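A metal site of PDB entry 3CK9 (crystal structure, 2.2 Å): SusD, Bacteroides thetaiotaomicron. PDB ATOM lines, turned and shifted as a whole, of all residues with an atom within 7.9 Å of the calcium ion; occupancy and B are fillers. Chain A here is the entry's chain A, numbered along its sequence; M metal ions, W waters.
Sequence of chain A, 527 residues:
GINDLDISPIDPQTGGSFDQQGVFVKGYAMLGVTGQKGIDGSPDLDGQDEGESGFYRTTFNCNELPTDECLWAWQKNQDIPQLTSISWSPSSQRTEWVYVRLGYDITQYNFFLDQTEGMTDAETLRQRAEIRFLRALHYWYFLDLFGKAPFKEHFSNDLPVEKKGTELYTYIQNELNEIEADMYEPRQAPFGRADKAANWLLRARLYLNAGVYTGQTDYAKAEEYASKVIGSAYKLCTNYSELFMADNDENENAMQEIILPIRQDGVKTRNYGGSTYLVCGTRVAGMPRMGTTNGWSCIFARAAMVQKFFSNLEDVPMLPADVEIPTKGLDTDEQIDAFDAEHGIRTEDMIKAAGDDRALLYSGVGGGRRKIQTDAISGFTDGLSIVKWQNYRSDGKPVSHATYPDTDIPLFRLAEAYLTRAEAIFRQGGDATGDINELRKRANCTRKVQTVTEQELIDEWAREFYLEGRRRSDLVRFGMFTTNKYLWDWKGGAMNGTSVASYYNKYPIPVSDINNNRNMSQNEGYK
OD2 of Asp 249 lies close to NH2 of Arg 263 (3.4 Å). The side-chain carboxylate of Asp 406 is in hydrogen-bond range of the backbone NH of Gly 266, 2.7 Å away. The side-chain carboxylate (OD1) of Asp 406 is in hydrogen-bond range of the side-chain hydroxyl (OG) of Ser 400, 2.5 Å away. N of Ser 275 lies within hydrogen-bond range of OE1 of Gln 264 (2.9 Å). The side-chain carboxylate (OD2) of Asp 408 lies within salt-bridge range of the guanidinium group (NE) of Arg 263, 2.8 Å away. O of Asp 408 sits at hydrogen-bond distance from ND2 of Asn 248 (2.8 Å).
The calcium ion is bound by the side-chain carboxylate (OD2) of Asp 249 (2.3 Å). Water W1 binds the calcium ion, at 2.3 Å. O of Asp 406 is bound to the calcium ion. The calcium ion is bound by O of Gln 264. OD1 of Asp 408 is bound to the calcium ion, 2.5 Å away. Water W3 binds the calcium ion (2.6 Å). Water W2 is bound to the calcium ion (2.7 Å).
Of the 22 residues printed, 4 come within 4 Å of the calcium ion. Along chain A the residues within 4 Å of the calcium ion span positions 249 to 408.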
ATOM      1  N   PHE A 191       6.167 -21.733 -16.242  1.00  0.00           N
ATOM      2  CA  PHE A 191       4.926 -22.005 -15.533  1.00  0.00           C
ATOM      3  C   PHE A 191       3.718 -21.687 -16.422  1.00  0.00           C
ATOM      4  O   PHE A 191       3.571 -20.575 -16.926  1.00  0.00           O
ATOM      5  CB  PHE A 191       4.864 -21.180 -14.243  1.00  0.00           C
ATOM      6  CG  PHE A 191       3.825 -21.660 -13.277  1.00  0.00           C
ATOM      7  CD1 PHE A 191       3.910 -22.935 -12.717  1.00  0.00           C
ATOM      8  CD2 PHE A 191       2.734 -20.859 -12.940  1.00  0.00           C
ATOM      9  CE1 PHE A 191       2.939 -23.400 -11.848  1.00  0.00           C
ATOM     10  CE2 PHE A 191       1.754 -21.321 -12.072  1.00  0.00           C
ATOM     11  CZ  PHE A 191       1.857 -22.603 -11.521  1.00  0.00           C
ATOM     12  N   MET A 245      -5.232 -20.584  -3.715  1.00  0.00           N
ATOM     13  CA  MET A 245      -5.185 -19.196  -3.311  1.00  0.00           C
ATOM     14  C   MET A 245      -4.615 -18.287  -4.412  1.00  0.00           C
ATOM     15  O   MET A 245      -4.050 -18.763  -5.394  1.00  0.00           O
ATOM     16  CB  MET A 245      -4.403 -19.076  -1.993  1.00  0.00           C
ATOM     17  CG  MET A 245      -5.180 -19.717  -0.835  1.00  0.00           C
ATOM     18  SD  MET A 245      -4.381 -19.674   0.798  1.00  0.00           S
ATOM     19  CE  MET A 245      -4.909 -18.060   1.401  1.00  0.00           C
ATOM     20  N   ALA A 246      -4.775 -16.983  -4.229  1.00  0.00           N
ATOM     21  CA  ALA A 246      -4.351 -15.986  -5.204  1.00  0.00           C
ATOM     22  C   ALA A 246      -2.884 -16.030  -5.634  1.00  0.00           C
ATOM     23  O   ALA A 246      -2.558 -15.670  -6.763  1.00  0.00           O
ATOM     24  CB  ALA A 246      -4.717 -14.587  -4.706  1.00  0.00           C
ATOM     25  N   ASP A 247      -2.002 -16.470  -4.751  1.00  0.00           N
ATOM     26  CA  ASP A 247      -0.582 -16.527  -5.072  1.00  0.00           C
ATOM     27  C   ASP A 247      -0.081 -17.915  -5.436  1.00  0.00           C
ATOM     28  O   ASP A 247       1.108 -18.229  -5.250  1.00  0.00           O
ATOM     29  CB  ASP A 247       0.244 -15.980  -3.909  1.00  0.00           C
ATOM     30  CG  ASP A 247      -0.002 -16.752  -2.611  1.00  0.00           C
ATOM     31  OD1 ASP A 247      -1.054 -17.401  -2.482  1.00  0.00           O
ATOM     32  OD2 ASP A 247       0.875 -16.675  -1.707  1.00  0.00           O
ATOM     33  N   ASN A 248      -0.972 -18.762  -5.962  1.00  0.00           N
ATOM     34  CA  ASN A 248      -0.551 -20.107  -6.334  1.00  0.00           C
ATOM     35  C   ASN A 248       0.334 -20.102  -7.583  1.00  0.00           C
ATOM     36  O   ASN A 248       0.743 -21.165  -8.053  1.00  0.00           O
ATOM     37  CB  ASN A 248      -1.761 -21.045  -6.502  1.00  0.00           C
ATOM     38  CG  ASN A 248      -2.756 -20.559  -7.533  1.00  0.00           C
ATOM     39  OD1 ASN A 248      -2.526 -19.575  -8.242  1.00  0.00           O
ATOM     40  ND2 ASN A 248      -3.886 -21.265  -7.640  1.00  0.00           N
ATOM     41  N   ASP A 249       0.634 -18.913  -8.113  1.00  0.00           N
ATOM     42  CA  ASP A 249       1.545 -18.789  -9.241  1.00  0.00           C
ATOM     43  C   ASP A 249       2.811 -18.049  -8.788  1.00  0.00           C
ATOM     44  O   ASP A 249       3.650 -17.677  -9.606  1.00  0.00           O
ATOM     45  CB  ASP A 249       0.895 -18.067 -10.449  1.00  0.00           C
ATOM     46  CG  ASP A 249       0.479 -16.655 -10.121  1.00  0.00           C
ATOM     47  OD1 ASP A 249       0.918 -16.108  -9.095  1.00  0.00           O
ATOM     48  OD2 ASP A 249      -0.281 -16.065 -10.929  1.00  0.00           O
ATOM     49  N   GLU A 250       2.929 -17.843  -7.485  1.00  0.00           N
ATOM     50  CA  GLU A 250       4.092 -17.183  -6.879  1.00  0.00           C
ATOM     51  C   GLU A 250       4.340 -17.756  -5.486  1.00  0.00           C
ATOM     52  O   GLU A 250       4.656 -17.025  -4.549  1.00  0.00           O
ATOM     53  CB  GLU A 250       3.883 -15.668  -6.800  1.00  0.00           C
ATOM     54  CG  GLU A 250       3.593 -15.008  -8.147  1.00  0.00           C
ATOM     55  CD  GLU A 250       3.389 -13.509  -8.039  1.00  0.00           C
ATOM     56  OE1 GLU A 250       3.109 -13.024  -6.931  1.00  0.00           O
ATOM     57  OE2 GLU A 250       3.508 -12.829  -9.076  1.00  0.00           O
ATOM     58  N   ILE A 262      -3.949 -23.171 -15.051  1.00  0.00           N
ATOM     59  CA  ILE A 262      -4.682 -22.394 -16.034  1.00  0.00           C
ATOM     60  C   ILE A 262      -4.504 -21.005 -15.477  1.00  0.00           C
ATOM     61  O   ILE A 262      -5.158 -20.622 -14.514  1.00  0.00           O
ATOM     62  CB  ILE A 262      -6.177 -22.770 -16.071  1.00  0.00           C
ATOM     63  CG1 ILE A 262      -6.334 -24.186 -16.650  1.00  0.00           C
ATOM     64  CG2 ILE A 262      -6.960 -21.742 -16.874  1.00  0.00           C
ATOM     65  CD1 ILE A 262      -7.787 -24.675 -16.704  1.00  0.00           C
ATOM     66  N   ARG A 263      -3.572 -20.260 -16.063  1.00  0.00           N
ATOM     67  CA  ARG A 263      -3.284 -18.916 -15.608  1.00  0.00           C
ATOM     68  C   ARG A 263      -4.540 -18.058 -15.570  1.00  0.00           C
ATOM     69  O   ARG A 263      -5.358 -18.093 -16.470  1.00  0.00           O
ATOM     70  CB  ARG A 263      -2.213 -18.272 -16.500  1.00  0.00           C
ATOM     71  CG  ARG A 263      -0.926 -19.099 -16.665  1.00  0.00           C
ATOM     72  CD  ARG A 263      -0.378 -19.589 -15.320  1.00  0.00           C
ATOM     73  NE  ARG A 263       0.062 -18.503 -14.442  1.00  0.00           N
ATOM     74  CZ  ARG A 263       1.192 -17.817 -14.597  1.00  0.00           C
ATOM     75  NH1 ARG A 263       2.016 -18.090 -15.608  1.00  0.00           N
ATOM     76  NH2 ARG A 263       1.501 -16.849 -13.751  1.00  0.00           N
ATOM     77  N   GLN A 264      -4.667 -17.286 -14.496  1.00  0.00           N
ATOM     78  CA  GLN A 264      -5.787 -16.387 -14.303  1.00  0.00           C
ATOM     79  C   GLN A 264      -5.216 -15.151 -13.611  1.00  0.00           C
ATOM     80  O   GLN A 264      -4.369 -15.266 -12.722  1.00  0.00           O
ATOM     81  CB  GLN A 264      -6.854 -17.021 -13.409  1.00  0.00           C
ATOM     82  CG  GLN A 264      -7.499 -18.256 -14.022  1.00  0.00           C
ATOM     83  CD  GLN A 264      -8.510 -17.922 -15.097  1.00  0.00           C
ATOM     84  OE1 GLN A 264      -9.679 -17.657 -14.815  1.00  0.00           O
ATOM     85  NE2 GLN A 264      -8.059 -17.932 -16.354  1.00  0.00           N
ATOM     86  N   ASP A 265      -5.659 -13.976 -14.025  1.00  0.00           N
ATOM     87  CA  ASP A 265      -5.165 -12.769 -13.407  1.00  0.00           C
ATOM     88  C   ASP A 265      -6.281 -11.749 -13.253  1.00  0.00           C
ATOM     89  O   ASP A 265      -7.082 -11.542 -14.174  1.00  0.00           O
ATOM     90  CB  ASP A 265      -4.009 -12.187 -14.222  1.00  0.00           C
ATOM     91  CG  ASP A 265      -3.461 -10.925 -13.609  1.00  0.00           C
ATOM     92  OD1 ASP A 265      -3.934  -9.828 -13.980  1.00  0.00           O
ATOM     93  OD2 ASP A 265      -2.566 -11.025 -12.728  1.00  0.00           O
ATOM     94  N   GLY A 266      -6.312 -11.119 -12.089  1.00  0.00           N
ATOM     95  CA  GLY A 266      -7.325 -10.142 -11.787  1.00  0.00           C
ATOM     96  C   GLY A 266      -7.399  -8.965 -12.736  1.00  0.00           C
ATOM     97  O   GLY A 266      -8.455  -8.361 -12.897  1.00  0.00           O
ATOM     98  N   LYS A 268      -5.254  -8.871 -16.013  1.00  0.00           N
ATOM     99  CA  LYS A 268      -4.973  -9.289 -17.386  1.00  0.00           C
ATOM    100  C   LYS A 268      -5.768 -10.471 -17.947  1.00  0.00           C
ATOM    101  O   LYS A 268      -6.225 -10.421 -19.085  1.00  0.00           O
ATOM    102  CB  LYS A 268      -3.482  -9.615 -17.537  1.00  0.00           C
ATOM    103  CG  LYS A 268      -2.544  -8.499 -17.099  1.00  0.00           C
ATOM    104  CD  LYS A 268      -1.103  -9.018 -17.036  1.00  0.00           C
ATOM    105  CE  LYS A 268      -0.968 -10.178 -16.053  1.00  0.00           C
ATOM    106  NZ  LYS A 268       0.430 -10.643 -15.916  1.00  0.00           N
ATOM    107  N   THR A 269      -5.920 -11.535 -17.163  1.00  0.00           N
ATOM    108  CA  THR A 269      -6.612 -12.732 -17.643  1.00  0.00           C
ATOM    109  C   THR A 269      -7.896 -13.033 -16.888  1.00  0.00           C
ATOM    110  O   THR A 269      -7.901 -13.804 -15.927  1.00  0.00           O
ATOM    111  CB  THR A 269      -5.680 -13.962 -17.526  1.00  0.00           C
ATOM    112  OG1 THR A 269      -4.387 -13.619 -18.048  1.00  0.00           O
ATOM    113  CG2 THR A 269      -6.218 -15.137 -18.313  1.00  0.00           C
ATOM    114  N   SER A 275     -11.422 -18.642 -12.717  1.00  0.00           N
ATOM    115  CA  SER A 275     -11.336 -18.663 -11.263  1.00  0.00           C
ATOM    116  C   SER A 275     -12.392 -17.725 -10.693  1.00  0.00           C
ATOM    117  O   SER A 275     -12.794 -17.864  -9.538  1.00  0.00           O
ATOM    118  CB  SER A 275      -9.943 -18.265 -10.775  1.00  0.00           C
ATOM    119  OG  SER A 275      -9.601 -16.944 -11.153  1.00  0.00           O
ATOM    120  N   ARG A 393      -3.918 -14.093  -0.979  1.00  0.00           N
ATOM    121  CA  ARG A 393      -2.585 -14.660  -1.122  1.00  0.00           C
ATOM    122  C   ARG A 393      -2.162 -15.253   0.222  1.00  0.00           C
ATOM    123  O   ARG A 393      -2.454 -14.684   1.276  1.00  0.00           O
ATOM    124  CB  ARG A 393      -1.579 -13.591  -1.540  1.00  0.00           C
ATOM    125  CG  ARG A 393      -1.794 -13.041  -2.944  1.00  0.00           C
ATOM    126  CD  ARG A 393      -0.773 -11.936  -3.238  1.00  0.00           C
ATOM    127  NE  ARG A 393       0.606 -12.421  -3.163  1.00  0.00           N
ATOM    128  CZ  ARG A 393       1.343 -12.753  -4.221  1.00  0.00           C
ATOM    129  NH1 ARG A 393       0.833 -12.642  -5.445  1.00  0.00           N
ATOM    130  NH2 ARG A 393       2.595 -13.153  -4.061  1.00  0.00           N
ATOM    131  N   SER A 400      -4.230  -8.269  -7.397  1.00  0.00           N
ATOM    132  CA  SER A 400      -4.269  -7.248  -8.439  1.00  0.00           C
ATOM    133  C   SER A 400      -5.603  -6.504  -8.602  1.00  0.00           C
ATOM    134  O   SER A 400      -5.616  -5.328  -8.949  1.00  0.00           O
ATOM    135  CB  SER A 400      -3.842  -7.844  -9.784  1.00  0.00           C
ATOM    136  OG  SER A 400      -4.858  -8.627 -10.357  1.00  0.00           O
ATOM    137  N   PRO A 405     -10.366 -12.450  -9.368  1.00  0.00           N
ATOM    138  CA  PRO A 405      -9.261 -13.140  -8.692  1.00  0.00           C
ATOM    139  C   PRO A 405      -7.995 -13.385  -9.502  1.00  0.00           C
ATOM    140  O   PRO A 405      -8.036 -13.531 -10.729  1.00  0.00           O
ATOM    141  CB  PRO A 405      -9.917 -14.442  -8.247  1.00  0.00           C
ATOM    142  CG  PRO A 405     -10.818 -14.737  -9.380  1.00  0.00           C
ATOM    143  CD  PRO A 405     -11.450 -13.391  -9.684  1.00  0.00           C
ATOM    144  N   ASP A 406      -6.858 -13.434  -8.804  1.00  0.00           N
ATOM    145  CA  ASP A 406      -5.567 -13.706  -9.416  1.00  0.00           C
ATOM    146  C   ASP A 406      -5.331 -15.209  -9.383  1.00  0.00           C
ATOM    147  O   ASP A 406      -4.437 -15.731 -10.062  1.00  0.00           O
ATOM    148  CB  ASP A 406      -4.429 -13.031  -8.639  1.00  0.00           C
ATOM    149  CG  ASP A 406      -4.429 -11.524  -8.768  1.00  0.00           C
ATOM    150  OD1 ASP A 406      -5.086 -10.997  -9.680  1.00  0.00           O
ATOM    151  OD2 ASP A 406      -3.748 -10.869  -7.950  1.00  0.00           O
ATOM    152  N   THR A 407      -6.140 -15.891  -8.589  1.00  0.00           N
ATOM    153  CA  THR A 407      -6.016 -17.331  -8.413  1.00  0.00           C
ATOM    154  C   THR A 407      -6.053 -18.162  -9.695  1.00  0.00           C
ATOM    155  O   THR A 407      -6.974 -18.047 -10.504  1.00  0.00           O
ATOM    156  CB  THR A 407      -7.108 -17.863  -7.481  1.00  0.00           C
ATOM    157  OG1 THR A 407      -7.119 -17.071  -6.284  1.00  0.00           O
ATOM    158  CG2 THR A 407      -6.826 -19.316  -7.113  1.00  0.00           C
ATOM    159  N   ASP A 408      -5.022 -18.986  -9.854  1.00  0.00           N
ATOM    160  CA  ASP A 408      -4.896 -19.871 -10.997  1.00  0.00           C
ATOM    161  C   ASP A 408      -5.678 -21.134 -10.691  1.00  0.00           C
ATOM    162  O   ASP A 408      -5.890 -21.476  -9.529  1.00  0.00           O
ATOM    163  CB  ASP A 408      -3.433 -20.265 -11.224  1.00  0.00           C
ATOM    164  CG  ASP A 408      -2.654 -19.217 -11.999  1.00  0.00           C
ATOM    165  OD1 ASP A 408      -3.208 -18.138 -12.302  1.00  0.00           O
ATOM    166  OD2 ASP A 408      -1.472 -19.475 -12.300  1.00  0.00           O
ATOM    167  N   ILE A 409      -6.107 -21.822 -11.738  1.00  0.00           N
ATOM    168  CA  ILE A 409      -6.823 -23.078 -11.561  1.00  0.00           C
ATOM    169  C   ILE A 409      -5.803 -24.205 -11.785  1.00  0.00           C
ATOM    170  O   ILE A 409      -5.314 -24.372 -12.894  1.00  0.00           O
ATOM    171  CB  ILE A 409      -7.956 -23.227 -12.607  1.00  0.00           C
ATOM    172  CG1 ILE A 409      -9.013 -22.138 -12.396  1.00  0.00           C
ATOM    173  CG2 ILE A 409      -8.580 -24.630 -12.500  1.00  0.00           C
ATOM    174  CD1 ILE A 409     -10.140 -22.162 -13.422  1.00  0.00           C
HETATM  175 CA    CA M   1      -2.516 -15.928 -11.368  1.00  0.00          CA
HETATM  176  O   HOH W   1      -2.092 -13.732 -10.802  1.00  0.00           O
HETATM  177  O   HOH W   2      -1.560 -15.141 -13.747  1.00  0.00           O
HETATM  178  O   HOH W   3      -2.394 -16.866  -8.934  1.00  0.00           O
